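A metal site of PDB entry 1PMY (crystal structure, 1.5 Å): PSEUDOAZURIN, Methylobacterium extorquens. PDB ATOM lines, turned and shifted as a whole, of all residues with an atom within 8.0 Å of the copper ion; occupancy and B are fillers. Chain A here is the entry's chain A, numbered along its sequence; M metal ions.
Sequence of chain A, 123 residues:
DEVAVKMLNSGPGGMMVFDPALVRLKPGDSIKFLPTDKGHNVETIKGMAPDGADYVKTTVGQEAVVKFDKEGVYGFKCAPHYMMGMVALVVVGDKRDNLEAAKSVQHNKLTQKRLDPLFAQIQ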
ATOM      1  N   MET A   7     -18.089 -22.541 -22.490  1.00  0.00           N
ATOM      2  CA  MET A   7     -18.540 -22.055 -21.146  1.00  0.00           C
ATOM      3  C   MET A   7     -17.776 -20.737 -20.874  1.00  0.00           C
ATOM      4  O   MET A   7     -16.537 -20.780 -20.698  1.00  0.00           O
ATOM      5  CB  MET A   7     -18.235 -23.180 -20.148  1.00  0.00           C
ATOM      6  CG  MET A   7     -19.112 -24.370 -20.610  1.00  0.00           C
ATOM      7  SD  MET A   7     -19.000 -25.698 -19.354  1.00  0.00           S
ATOM      8  CE  MET A   7     -17.254 -26.035 -19.529  1.00  0.00           C
ATOM      9  N   LEU A   8     -18.507 -19.665 -20.927  1.00  0.00           N
ATOM     10  CA  LEU A   8     -17.897 -18.309 -20.835  1.00  0.00           C
ATOM     11  C   LEU A   8     -18.388 -17.414 -19.695  1.00  0.00           C
ATOM     12  O   LEU A   8     -19.514 -17.404 -19.317  1.00  0.00           O
ATOM     13  CB  LEU A   8     -18.223 -17.548 -22.149  1.00  0.00           C
ATOM     14  CG  LEU A   8     -17.765 -18.124 -23.459  1.00  0.00           C
ATOM     15  CD1 LEU A   8     -18.590 -17.601 -24.630  1.00  0.00           C
ATOM     16  CD2 LEU A   8     -16.310 -18.022 -23.675  1.00  0.00           C
ATOM     17  N   ASN A   9     -17.386 -16.687 -19.212  1.00  0.00           N
ATOM     18  CA  ASN A   9     -17.664 -15.605 -18.228  1.00  0.00           C
ATOM     19  C   ASN A   9     -18.432 -14.464 -18.926  1.00  0.00           C
ATOM     20  O   ASN A   9     -19.319 -13.819 -18.279  1.00  0.00           O
ATOM     21  CB  ASN A   9     -16.361 -15.101 -17.621  1.00  0.00           C
ATOM     22  CG  ASN A   9     -15.683 -16.045 -16.710  1.00  0.00           C
ATOM     23  OD1 ASN A   9     -16.227 -17.139 -16.326  1.00  0.00           O
ATOM     24  ND2 ASN A   9     -14.515 -15.661 -16.222  1.00  0.00           N
ATOM     25  N   MET A  15     -22.967 -11.745 -19.075  1.00  0.00           N
ATOM     26  CA  MET A  15     -22.164 -12.499 -18.153  1.00  0.00           C
ATOM     27  C   MET A  15     -22.685 -13.926 -17.907  1.00  0.00           C
ATOM     28  O   MET A  15     -23.895 -14.120 -17.799  1.00  0.00           O
ATOM     29  CB  MET A  15     -21.896 -11.871 -16.798  1.00  0.00           C
ATOM     30  CG  MET A  15     -21.672 -10.393 -16.801  1.00  0.00           C
ATOM     31  SD  MET A  15     -20.478  -9.893 -18.066  1.00  0.00           S
ATOM     32  CE  MET A  15     -18.960 -10.631 -17.478  1.00  0.00           C
ATOM     33  N   MET A  16     -21.767 -14.856 -17.843  1.00  0.00           N
ATOM     34  CA  MET A  16     -22.043 -16.282 -17.518  1.00  0.00           C
ATOM     35  C   MET A  16     -22.994 -16.899 -18.541  1.00  0.00           C
ATOM     36  O   MET A  16     -24.218 -17.074 -18.235  1.00  0.00           O
ATOM     37  CB  MET A  16     -22.517 -16.445 -16.111  1.00  0.00           C
ATOM     38  CG  MET A  16     -21.812 -15.645 -15.057  1.00  0.00           C
ATOM     39  SD  MET A  16     -20.061 -16.215 -15.108  1.00  0.00           S
ATOM     40  CE  MET A  16     -19.393 -15.206 -13.819  1.00  0.00           C
ATOM     41  N   VAL A  17     -22.492 -17.219 -19.698  1.00  0.00           N
ATOM     42  CA  VAL A  17     -23.212 -17.777 -20.806  1.00  0.00           C
ATOM     43  C   VAL A  17     -22.529 -19.017 -21.488  1.00  0.00           C
ATOM     44  O   VAL A  17     -21.331 -19.254 -21.349  1.00  0.00           O
ATOM     45  CB  VAL A  17     -23.462 -16.713 -21.913  1.00  0.00           C
ATOM     46  CG1 VAL A  17     -24.095 -15.423 -21.366  1.00  0.00           C
ATOM     47  CG2 VAL A  17     -22.157 -16.350 -22.604  1.00  0.00           C
ATOM     48  N   PHE A  18     -23.410 -19.780 -22.121  1.00  0.00           N
ATOM     49  CA  PHE A  18     -23.034 -20.902 -22.944  1.00  0.00           C
ATOM     50  C   PHE A  18     -23.102 -20.272 -24.358  1.00  0.00           C
ATOM     51  O   PHE A  18     -24.053 -19.524 -24.607  1.00  0.00           O
ATOM     52  CB  PHE A  18     -23.937 -22.125 -22.847  1.00  0.00           C
ATOM     53  CG  PHE A  18     -23.805 -22.927 -21.593  1.00  0.00           C
ATOM     54  CD1 PHE A  18     -22.809 -23.880 -21.356  1.00  0.00           C
ATOM     55  CD2 PHE A  18     -24.860 -22.817 -20.663  1.00  0.00           C
ATOM     56  CE1 PHE A  18     -22.816 -24.640 -20.168  1.00  0.00           C
ATOM     57  CE2 PHE A  18     -24.831 -23.549 -19.469  1.00  0.00           C
ATOM     58  CZ  PHE A  18     -23.823 -24.417 -19.180  1.00  0.00           C
ATOM     59  N   ASP A  37     -13.506 -20.585 -20.218  1.00  0.00           N
ATOM     60  CA  ASP A  37     -13.215 -19.922 -18.938  1.00  0.00           C
ATOM     61  C   ASP A  37     -13.432 -21.045 -17.910  1.00  0.00           C
ATOM     62  O   ASP A  37     -14.220 -21.980 -18.114  1.00  0.00           O
ATOM     63  CB  ASP A  37     -14.124 -18.743 -18.683  1.00  0.00           C
ATOM     64  CG  ASP A  37     -13.841 -17.534 -19.574  1.00  0.00           C
ATOM     65  OD1 ASP A  37     -12.682 -17.146 -19.663  1.00  0.00           O
ATOM     66  OD2 ASP A  37     -14.753 -16.913 -20.098  1.00  0.00           O
ATOM     67  N   LYS A  38     -12.666 -20.978 -16.855  1.00  0.00           N
ATOM     68  CA  LYS A  38     -12.743 -21.938 -15.757  1.00  0.00           C
ATOM     69  C   LYS A  38     -13.985 -21.602 -14.888  1.00  0.00           C
ATOM     70  O   LYS A  38     -14.498 -20.484 -14.900  1.00  0.00           O
ATOM     71  CB  LYS A  38     -11.459 -21.650 -14.921  1.00  0.00           C
ATOM     72  CG  LYS A  38     -11.538 -21.576 -13.462  1.00  0.00           C
ATOM     73  CD  LYS A  38     -10.663 -20.690 -12.643  1.00  0.00           C
ATOM     74  CE  LYS A  38     -10.686 -19.216 -13.102  1.00  0.00           C
ATOM     75  NZ  LYS A  38     -11.661 -18.435 -12.271  1.00  0.00           N
ATOM     76  N   GLY A  39     -14.279 -22.599 -14.037  1.00  0.00           N
ATOM     77  CA  GLY A  39     -15.340 -22.377 -13.020  1.00  0.00           C
ATOM     78  C   GLY A  39     -16.764 -22.641 -13.537  1.00  0.00           C
ATOM     79  O   GLY A  39     -17.664 -22.163 -12.853  1.00  0.00           O
ATOM     80  N   HIS A  40     -16.914 -23.273 -14.650  1.00  0.00           N
ATOM     81  CA  HIS A  40     -18.263 -23.603 -15.188  1.00  0.00           C
ATOM     82  C   HIS A  40     -18.479 -25.101 -15.227  1.00  0.00           C
ATOM     83  O   HIS A  40     -17.488 -25.842 -15.315  1.00  0.00           O
ATOM     84  CB  HIS A  40     -18.503 -22.906 -16.507  1.00  0.00           C
ATOM     85  CG  HIS A  40     -18.341 -21.441 -16.510  1.00  0.00           C
ATOM     86  ND1 HIS A  40     -19.114 -20.446 -15.971  1.00  0.00           N
ATOM     87  CD2 HIS A  40     -17.277 -20.760 -17.096  1.00  0.00           C
ATOM     88  CE1 HIS A  40     -18.614 -19.268 -16.210  1.00  0.00           C
ATOM     89  NE2 HIS A  40     -17.525 -19.431 -16.902  1.00  0.00           N
ATOM     90  N   ASN A  41     -19.762 -25.505 -15.168  1.00  0.00           N
ATOM     91  CA  ASN A  41     -20.066 -26.961 -15.388  1.00  0.00           C
ATOM     92  C   ASN A  41     -21.383 -26.969 -16.208  1.00  0.00           C
ATOM     93  O   ASN A  41     -21.962 -25.918 -16.514  1.00  0.00           O
ATOM     94  CB  ASN A  41     -20.061 -27.872 -14.222  1.00  0.00           C
ATOM     95  CG  ASN A  41     -21.305 -27.751 -13.314  1.00  0.00           C
ATOM     96  OD1 ASN A  41     -21.993 -26.712 -13.484  1.00  0.00           O
ATOM     97  ND2 ASN A  41     -21.557 -28.884 -12.689  1.00  0.00           N
ATOM     98  N   VAL A  42     -21.882 -28.189 -16.319  1.00  0.00           N
ATOM     99  CA  VAL A  42     -23.156 -28.463 -16.975  1.00  0.00           C
ATOM    100  C   VAL A  42     -23.935 -29.491 -16.090  1.00  0.00           C
ATOM    101  O   VAL A  42     -23.398 -30.519 -15.604  1.00  0.00           O
ATOM    102  CB  VAL A  42     -22.871 -29.117 -18.392  1.00  0.00           C
ATOM    103  CG1 VAL A  42     -24.251 -29.199 -19.100  1.00  0.00           C
ATOM    104  CG2 VAL A  42     -22.053 -28.112 -19.251  1.00  0.00           C
ATOM    105  N   VAL A  60     -16.694 -29.233 -12.492  1.00  0.00           N
ATOM    106  CA  VAL A  60     -16.363 -27.836 -12.739  1.00  0.00           C
ATOM    107  C   VAL A  60     -14.938 -27.640 -13.356  1.00  0.00           C
ATOM    108  O   VAL A  60     -13.983 -28.273 -12.862  1.00  0.00           O
ATOM    109  CB  VAL A  60     -16.684 -26.996 -11.530  1.00  0.00           C
ATOM    110  CG1 VAL A  60     -16.111 -25.568 -11.726  1.00  0.00           C
ATOM    111  CG2 VAL A  60     -18.141 -26.903 -11.154  1.00  0.00           C
ATOM    112  N   LYS A  77     -28.130 -26.234 -16.908  1.00  0.00           N
ATOM    113  CA  LYS A  77     -27.626 -25.070 -16.157  1.00  0.00           C
ATOM    114  C   LYS A  77     -26.119 -25.342 -15.918  1.00  0.00           C
ATOM    115  O   LYS A  77     -25.566 -26.421 -16.007  1.00  0.00           O
ATOM    116  CB  LYS A  77     -28.344 -25.039 -14.761  1.00  0.00           C
ATOM    117  CG  LYS A  77     -28.092 -26.144 -13.775  1.00  0.00           C
ATOM    118  CD  LYS A  77     -28.818 -25.809 -12.424  1.00  0.00           C
ATOM    119  CE  LYS A  77     -28.675 -27.009 -11.518  1.00  0.00           C
ATOM    120  NZ  LYS A  77     -29.336 -26.578 -10.207  1.00  0.00           N
ATOM    121  N   CYS A  78     -25.503 -24.197 -15.566  1.00  0.00           N
ATOM    122  CA  CYS A  78     -24.157 -24.185 -14.985  1.00  0.00           C
ATOM    123  C   CYS A  78     -24.475 -24.119 -13.469  1.00  0.00           C
ATOM    124  O   CYS A  78     -25.157 -23.127 -13.076  1.00  0.00           O
ATOM    125  CB  CYS A  78     -23.311 -23.007 -15.488  1.00  0.00           C
ATOM    126  SG  CYS A  78     -21.940 -22.781 -14.366  1.00  0.00           S
ATOM    127  N   ALA A  79     -24.201 -25.171 -12.701  1.00  0.00           N
ATOM    128  CA  ALA A  79     -24.556 -25.124 -11.268  1.00  0.00           C
ATOM    129  C   ALA A  79     -24.206 -23.931 -10.491  1.00  0.00           C
ATOM    130  O   ALA A  79     -25.139 -23.245  -9.956  1.00  0.00           O
ATOM    131  CB  ALA A  79     -24.559 -26.439 -10.573  1.00  0.00           C
ATOM    132  N   PRO A  80     -22.934 -23.518 -10.417  1.00  0.00           N
ATOM    133  CA  PRO A  80     -22.512 -22.350  -9.654  1.00  0.00           C
ATOM    134  C   PRO A  80     -23.116 -21.051 -10.236  1.00  0.00           C
ATOM    135  O   PRO A  80     -23.321 -20.148  -9.367  1.00  0.00           O
ATOM    136  CB  PRO A  80     -21.010 -22.279  -9.850  1.00  0.00           C
ATOM    137  CG  PRO A  80     -20.659 -23.254 -10.895  1.00  0.00           C
ATOM    138  CD  PRO A  80     -21.787 -24.322 -11.007  1.00  0.00           C
ATOM    139  N   HIS A  81     -23.471 -20.981 -11.552  1.00  0.00           N
ATOM    140  CA  HIS A  81     -24.032 -19.723 -12.058  1.00  0.00           C
ATOM    141  C   HIS A  81     -25.475 -19.776 -12.495  1.00  0.00           C
ATOM    142  O   HIS A  81     -25.903 -19.014 -13.401  1.00  0.00           O
ATOM    143  CB  HIS A  81     -23.171 -19.130 -13.276  1.00  0.00           C
ATOM    144  CG  HIS A  81     -21.735 -19.089 -12.883  1.00  0.00           C
ATOM    145  ND1 HIS A  81     -20.723 -19.728 -13.614  1.00  0.00           N
ATOM    146  CD2 HIS A  81     -21.149 -18.447 -11.839  1.00  0.00           C
ATOM    147  CE1 HIS A  81     -19.558 -19.447 -12.978  1.00  0.00           C
ATOM    148  NE2 HIS A  81     -19.773 -18.678 -11.964  1.00  0.00           N
ATOM    149  N   TYR A  82     -26.276 -20.698 -11.967  1.00  0.00           N
ATOM    150  CA  TYR A  82     -27.719 -20.771 -12.362  1.00  0.00           C
ATOM    151  C   TYR A  82     -28.497 -19.503 -12.018  1.00  0.00           C
ATOM    152  O   TYR A  82     -29.191 -18.981 -12.896  1.00  0.00           O
ATOM    153  CB  TYR A  82     -28.267 -22.079 -11.747  1.00  0.00           C
ATOM    154  CG  TYR A  82     -29.784 -22.176 -11.916  1.00  0.00           C
ATOM    155  CD1 TYR A  82     -30.433 -22.250 -13.135  1.00  0.00           C
ATOM    156  CD2 TYR A  82     -30.561 -21.996 -10.766  1.00  0.00           C
ATOM    157  CE1 TYR A  82     -31.846 -22.305 -13.212  1.00  0.00           C
ATOM    158  CE2 TYR A  82     -31.971 -21.968 -10.835  1.00  0.00           C
ATOM    159  CZ  TYR A  82     -32.598 -22.231 -12.026  1.00  0.00           C
ATOM    160  OH  TYR A  82     -33.972 -22.083 -12.066  1.00  0.00           O
ATOM    161  N   MET A  84     -27.410 -16.604 -11.891  1.00  0.00           N
ATOM    162  CA  MET A  84     -26.886 -15.671 -12.844  1.00  0.00           C
ATOM    163  C   MET A  84     -27.331 -15.959 -14.284  1.00  0.00           C
ATOM    164  O   MET A  84     -26.911 -15.263 -15.168  1.00  0.00           O
ATOM    165  CB  MET A  84     -25.330 -15.628 -12.785  1.00  0.00           C
ATOM    166  CG  MET A  84     -24.967 -14.807 -11.537  1.00  0.00           C
ATOM    167  SD  MET A  84     -23.118 -14.763 -11.486  1.00  0.00           S
ATOM    168  CE  MET A  84     -22.908 -13.346 -12.673  1.00  0.00           C
ATOM    169  N   GLY A  85     -28.258 -16.882 -14.512  1.00  0.00           N
ATOM    170  CA  GLY A  85     -28.812 -17.151 -15.808  1.00  0.00           C
ATOM    171  C   GLY A  85     -27.953 -17.977 -16.747  1.00  0.00           C
ATOM    172  O   GLY A  85     -28.262 -17.938 -17.965  1.00  0.00           O
ATOM    173  N   MET A  86     -26.990 -18.741 -16.211  1.00  0.00           N
ATOM    174  CA  MET A  86     -26.164 -19.544 -17.217  1.00  0.00           C
ATOM    175  C   MET A  86     -26.877 -20.852 -17.505  1.00  0.00           C
ATOM    176  O   MET A  86     -26.799 -21.822 -16.702  1.00  0.00           O
ATOM    177  CB  MET A  86     -24.781 -19.809 -16.580  1.00  0.00           C
ATOM    178  CG  MET A  86     -23.864 -20.216 -17.760  1.00  0.00           C
ATOM    179  SD  MET A  86     -22.098 -20.084 -17.190  1.00  0.00           S
ATOM    180  CE  MET A  86     -21.354 -21.110 -18.502  1.00  0.00           C
ATOM    181  N   VAL A  87     -27.631 -20.896 -18.572  1.00  0.00           N
ATOM    182  CA  VAL A  87     -28.470 -21.986 -19.042  1.00  0.00           C
ATOM    183  C   VAL A  87     -28.357 -22.197 -20.542  1.00  0.00           C
ATOM    184  O   VAL A  87     -28.025 -21.221 -21.254  1.00  0.00           O
ATOM    185  CB  VAL A  87     -29.970 -21.738 -18.583  1.00  0.00           C
ATOM    186  CG1 VAL A  87     -30.074 -21.853 -17.073  1.00  0.00           C
ATOM    187  CG2 VAL A  87     -30.456 -20.362 -19.078  1.00  0.00           C
HETATM  188 CU    CU M   1     -20.860 -21.055 -15.052  1.00  0.00          CU
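The side-chain sulfur of Cys 78 lies close to the backbone NH of Asn 41.
A ring nitrogen (NE2) of His 40 sits at hydrogen-bond distance from the side-chain amide oxygen (OD1) of Asn 9.
The copper ion is bound by a ring nitrogen (ND1) of His 81 (2.0 Å), a ring nitrogen (ND1) of His 40 (2.1 Å), the side-chain sulfur (SG) of Cys 78 (2.1 Å) and the side-chain sulfur (SD) of Met 86 (2.7 Å).
The copper ion has four donor atoms within binding distance.
The nearest printed residue that does not touch the copper ion is Gly 39 (4.03 Å).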
